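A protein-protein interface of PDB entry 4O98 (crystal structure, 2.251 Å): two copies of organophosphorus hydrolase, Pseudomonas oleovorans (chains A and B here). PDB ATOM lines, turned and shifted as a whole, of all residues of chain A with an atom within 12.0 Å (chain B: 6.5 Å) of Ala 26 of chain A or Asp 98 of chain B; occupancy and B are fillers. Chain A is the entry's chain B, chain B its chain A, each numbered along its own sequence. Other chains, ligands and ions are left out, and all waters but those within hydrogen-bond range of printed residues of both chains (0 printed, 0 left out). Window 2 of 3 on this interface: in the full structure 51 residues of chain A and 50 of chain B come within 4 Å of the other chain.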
ATOM      1  N   ALA A  26      -2.635   1.708 -18.002  1.00  0.00           N
ATOM      2  CA  ALA A  26      -3.730   1.144 -18.801  1.00  0.00           C
ATOM      3  C   ALA A  26      -4.135  -0.210 -18.257  1.00  0.00           C
ATOM      4  O   ALA A  26      -3.291  -0.948 -17.752  1.00  0.00           O
ATOM      5  CB  ALA A  26      -3.314   1.007 -20.268  1.00  0.00           C
ATOM      6  N   PRO A  27      -5.424  -0.562 -18.379  1.00  0.00           N
ATOM      7  CA  PRO A  27      -5.823  -1.906 -17.944  1.00  0.00           C
ATOM      8  C   PRO A  27      -5.140  -2.975 -18.802  1.00  0.00           C
ATOM      9  O   PRO A  27      -4.395  -2.644 -19.737  1.00  0.00           O
ATOM     10  CB  PRO A  27      -7.335  -1.921 -18.186  1.00  0.00           C
ATOM     11  CG  PRO A  27      -7.555  -0.906 -19.282  1.00  0.00           C
ATOM     12  CD  PRO A  27      -6.532   0.176 -19.018  1.00  0.00           C
ATOM     13  N   ALA A  28      -5.375  -4.244 -18.484  1.00  0.00           N
ATOM     14  CA  ALA A  28      -4.771  -5.318 -19.252  1.00  0.00           C
ATOM     15  C   ALA A  28      -5.305  -5.263 -20.674  1.00  0.00           C
ATOM     16  O   ALA A  28      -6.429  -4.814 -20.902  1.00  0.00           O
ATOM     17  CB  ALA A  28      -5.083  -6.656 -18.621  1.00  0.00           C
ATOM     18  N   GLN A  29      -4.504  -5.703 -21.634  1.00  0.00           N
ATOM     19  CA  GLN A  29      -4.981  -5.776 -23.013  1.00  0.00           C
ATOM     20  C   GLN A  29      -6.000  -6.916 -23.139  1.00  0.00           C
ATOM     21  O   GLN A  29      -5.860  -7.945 -22.491  1.00  0.00           O
ATOM     22  CB  GLN A  29      -3.805  -5.942 -23.980  1.00  0.00           C
ATOM     23  CG  GLN A  29      -2.769  -4.814 -23.863  1.00  0.00           C
ATOM     24  CD  GLN A  29      -1.598  -4.993 -24.811  1.00  0.00           C
ATOM     25  OE1 GLN A  29      -1.304  -6.105 -25.226  1.00  0.00           O
ATOM     26  NE2 GLN A  29      -0.933  -3.894 -25.166  1.00  0.00           N
ATOM     27  N   GLN A  30      -7.039  -6.714 -23.943  1.00  0.00           N
ATOM     28  CA  GLN A  30      -8.073  -7.729 -24.134  1.00  0.00           C
ATOM     29  C   GLN A  30      -7.610  -8.857 -25.044  1.00  0.00           C
ATOM     30  O   GLN A  30      -7.963 -10.018 -24.822  1.00  0.00           O
ATOM     31  CB  GLN A  30      -9.349  -7.098 -24.697  1.00  0.00           C
ATOM     32  CG  GLN A  30     -10.104  -6.253 -23.679  1.00  0.00           C
ATOM     33  CD  GLN A  30     -10.669  -7.097 -22.554  1.00  0.00           C
ATOM     34  OE1 GLN A  30     -11.403  -8.060 -22.796  1.00  0.00           O
ATOM     35  NE2 GLN A  30     -10.324  -6.747 -21.317  1.00  0.00           N
ATOM     36  N   LYS A  31      -6.859  -8.493 -26.085  1.00  0.00           N
ATOM     37  CA  LYS A  31      -6.200  -9.435 -27.004  1.00  0.00           C
ATOM     38  C   LYS A  31      -7.134 -10.221 -27.923  1.00  0.00           C
ATOM     39  O   LYS A  31      -6.805 -10.458 -29.081  1.00  0.00           O
ATOM     40  CB  LYS A  31      -5.290 -10.407 -26.251  1.00  0.00           C
ATOM     41  CG  LYS A  31      -4.179  -9.739 -25.460  1.00  0.00           C
ATOM     42  CD  LYS A  31      -3.411 -10.777 -24.638  1.00  0.00           C
ATOM     43  CE  LYS A  31      -2.260 -10.131 -23.877  1.00  0.00           C
ATOM     44  NZ  LYS A  31      -1.292 -11.141 -23.345  1.00  0.00           N
ATOM     45  N   ASN B  95      -4.287   0.454 -26.866  1.00  0.00           N
ATOM     46  CA  ASN B  95      -3.786   0.140 -25.536  1.00  0.00           C
ATOM     47  C   ASN B  95      -2.280  -0.055 -25.636  1.00  0.00           C
ATOM     48  O   ASN B  95      -1.822  -1.060 -26.181  1.00  0.00           O
ATOM     49  CB  ASN B  95      -4.459  -1.135 -25.003  1.00  0.00           C
ATOM     50  CG  ASN B  95      -4.152  -1.392 -23.534  1.00  0.00           C
ATOM     51  OD1 ASN B  95      -3.108  -0.982 -23.029  1.00  0.00           O
ATOM     52  ND2 ASN B  95      -5.068  -2.066 -22.840  1.00  0.00           N
ATOM     53  N   THR B  96      -1.521   0.909 -25.116  1.00  0.00           N
ATOM     54  CA  THR B  96      -0.057   0.880 -25.167  1.00  0.00           C
ATOM     55  C   THR B  96       0.587   0.237 -23.936  1.00  0.00           C
ATOM     56  O   THR B  96       1.798   0.049 -23.908  1.00  0.00           O
ATOM     57  CB  THR B  96       0.534   2.312 -25.284  1.00  0.00           C
ATOM     58  OG1 THR B  96       0.133   3.101 -24.154  1.00  0.00           O
ATOM     59  CG2 THR B  96       0.067   2.994 -26.558  1.00  0.00           C
ATOM     60  N   GLY B  97      -0.215  -0.090 -22.925  1.00  0.00           N
ATOM     61  CA  GLY B  97       0.321  -0.517 -21.641  1.00  0.00           C
ATOM     62  C   GLY B  97       0.336   0.643 -20.648  1.00  0.00           C
ATOM     63  O   GLY B  97      -0.154   0.524 -19.521  1.00  0.00           O
ATOM     64  N   ASP B  98       0.885   1.779 -21.075  1.00  0.00           N
ATOM     65  CA  ASP B  98       0.859   2.989 -20.261  1.00  0.00           C
ATOM     66  C   ASP B  98      -0.467   3.753 -20.375  1.00  0.00           C
ATOM     67  O   ASP B  98      -0.921   4.376 -19.410  1.00  0.00           O
ATOM     68  CB  ASP B  98       2.013   3.908 -20.648  1.00  0.00           C
ATOM     69  CG  ASP B  98       3.366   3.284 -20.378  1.00  0.00           C
ATOM     70  OD1 ASP B  98       3.457   2.411 -19.483  1.00  0.00           O
ATOM     71  OD2 ASP B  98       4.338   3.672 -21.065  1.00  0.00           O
ATOM     72  N   ASN B  99      -1.083   3.716 -21.554  1.00  0.00           N
ATOM     73  CA  ASN B  99      -2.339   4.441 -21.766  1.00  0.00           C
ATOM     74  C   ASN B  99      -3.370   3.654 -22.561  1.00  0.00           C
ATOM     75  O   ASN B  99      -3.025   2.860 -23.443  1.00  0.00           O
ATOM     76  CB  ASN B  99      -2.091   5.754 -22.506  1.00  0.00           C
ATOM     77  CG  ASN B  99      -1.230   6.707 -21.732  1.00  0.00           C
ATOM     78  OD1 ASN B  99      -0.005   6.608 -21.759  1.00  0.00           O
ATOM     79  ND2 ASN B  99      -1.862   7.657 -21.045  1.00  0.00           N
ATOM     80  N   LEU B 100      -4.637   3.885 -22.251  1.00  0.00           N
ATOM     81  CA  LEU B 100      -5.698   3.420 -23.132  1.00  0.00           C
ATOM     82  C   LEU B 100      -6.188   4.644 -23.900  1.00  0.00           C
ATOM     83  O   LEU B 100      -6.948   5.470 -23.363  1.00  0.00           O
ATOM     84  CB  LEU B 100      -6.840   2.781 -22.342  1.00  0.00           C
ATOM     85  CG  LEU B 100      -7.924   2.169 -23.225  1.00  0.00           C
ATOM     86  CD1 LEU B 100      -7.313   1.080 -24.084  1.00  0.00           C
ATOM     87  CD2 LEU B 100      -9.054   1.599 -22.387  1.00  0.00           C
ATOM     88  N   GLN B 131     -12.376   3.435 -18.683  1.00  0.00           N
ATOM     89  CA  GLN B 131     -10.946   3.105 -18.680  1.00  0.00           C
ATOM     90  C   GLN B 131     -10.120   3.994 -19.604  1.00  0.00           C
ATOM     91  O   GLN B 131      -8.889   3.976 -19.568  1.00  0.00           O
ATOM     92  CB  GLN B 131     -10.742   1.645 -19.064  1.00  0.00           C
ATOM     93  CG  GLN B 131     -11.535   0.688 -18.213  1.00  0.00           C
ATOM     94  CD  GLN B 131     -11.436  -0.735 -18.706  1.00  0.00           C
ATOM     95  OE1 GLN B 131     -11.650  -1.014 -19.887  1.00  0.00           O
ATOM     96  NE2 GLN B 131     -11.119  -1.648 -17.804  1.00  0.00           N
ATOM     97  N   ASP B 133      -8.194   6.909 -20.715  1.00  0.00           N
ATOM     98  CA  ASP B 133      -7.563   8.044 -20.062  1.00  0.00           C
ATOM     99  C   ASP B 133      -7.282   9.197 -21.027  1.00  0.00           C
ATOM    100  O   ASP B 133      -7.164  10.349 -20.605  1.00  0.00           O
ATOM    101  CB  ASP B 133      -6.279   7.618 -19.351  1.00  0.00           C
ATOM    102  CG  ASP B 133      -5.299   6.936 -20.277  1.00  0.00           C
ATOM    103  OD1 ASP B 133      -4.603   7.630 -21.048  1.00  0.00           O
ATOM    104  OD2 ASP B 133      -5.213   5.698 -20.221  1.00  0.00           O
ATOM    105  N   PRO B 216       4.138   8.498 -24.674  1.00  0.00           N
ATOM    106  CA  PRO B 216       5.239   7.644 -25.114  1.00  0.00           C
ATOM    107  C   PRO B 216       4.775   6.837 -26.321  1.00  0.00           C
ATOM    108  O   PRO B 216       3.694   6.249 -26.281  1.00  0.00           O
ATOM    109  CB  PRO B 216       5.493   6.732 -23.904  1.00  0.00           C
ATOM    110  CG  PRO B 216       4.324   6.948 -22.966  1.00  0.00           C
ATOM    111  CD  PRO B 216       3.816   8.317 -23.246  1.00  0.00           C
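Of chain A, only Ala 26 (3.5 Å) comes within 4 Å of Asp 98 of chain B.
No residue of chain A comes within 4 Å of Thr 96 of chain B.
Asn 99 of chain B touches just one residue of chain A: Ala 26 (3.5 Å).
No residue of chain A comes within 4 Å of Pro 216 of chain B.
Of the printed residues of chain B, Gln 29 of chain A touches Asn 95 (3.1 Å).
Printed residues of chain B within 4 Å of Pro 27 of chain A: Asn 95 and Gln 131.
No position is printed for both chains.
Of the 9 pairs that touch across the chains among the printed residues, none has its exchanged pair printed and touching as well.
The backbone carbonyl oxygen (O) of Asn 95 of chain B lies within hydrogen-bond range of the side-chain amide nitrogen (NE2) of Gln 29 of chain A.
The side-chain amide nitrogen of Asn 95 of chain B is in hydrogen-bond range of the backbone carbonyl oxygen of Pro 27 of chain A, 3.2 Å away.
The backbone carbonyl oxygen of Gly 97 of chain B is in hydrogen-bond range of the backbone NH of Ala 26 of chain A, 3.1 Å away.
The backbone NH (N) of Ala 26 of chain A is in hydrogen-bond range of the backbone carbonyl oxygen (O) of Asp 98 of chain B (3.5 Å).
The side-chain amide nitrogen (ND2) of Asn 99 of chain B sits at hydrogen-bond distance from the side-chain carboxylate (OD1) of Asp 133 of chain B.
The side-chain amide oxygen of Asn 95 of chain B lies within hydrogen-bond range of the backbone NH of Gly 97 of chain B (3.0 Å).
The backbone NH (N) of Leu 100 of chain B is in hydrogen-bond range of the side-chain carboxylate (OD2) of Asp 133 of chain B.
OG1 of Thr 96 of chain B sits close to N of Asp 98 of chain B (3.4 Å).
OG1 of Thr 96 of chain B is in hydrogen-bond range of N of Asn 99 of chain B (2.9 Å).
Among the printed residues, merely in contact across the chains: Ala 26 of chain A with Asn 95 of chain B, Ala 26 of chain A with Asn 99 of chain B, Ala 28 of chain A with Asn 95 of chain B, Ala 26 of chain A with Leu 100 of chain B and Pro 27 of chain A with Gln 131 of chain B.
Hydrophobic or aromatic side chains of chain A that line the printed part of chain B: Ala 26 and Pro 27.
Along chain A the printed residues that touch a printed residue of chain B span positions 26 to 29.
Of the 9 printed residues of chain B, 6 touch a printed residue of chain A.
Among the printed residues, 9 pairs touch across the chains.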
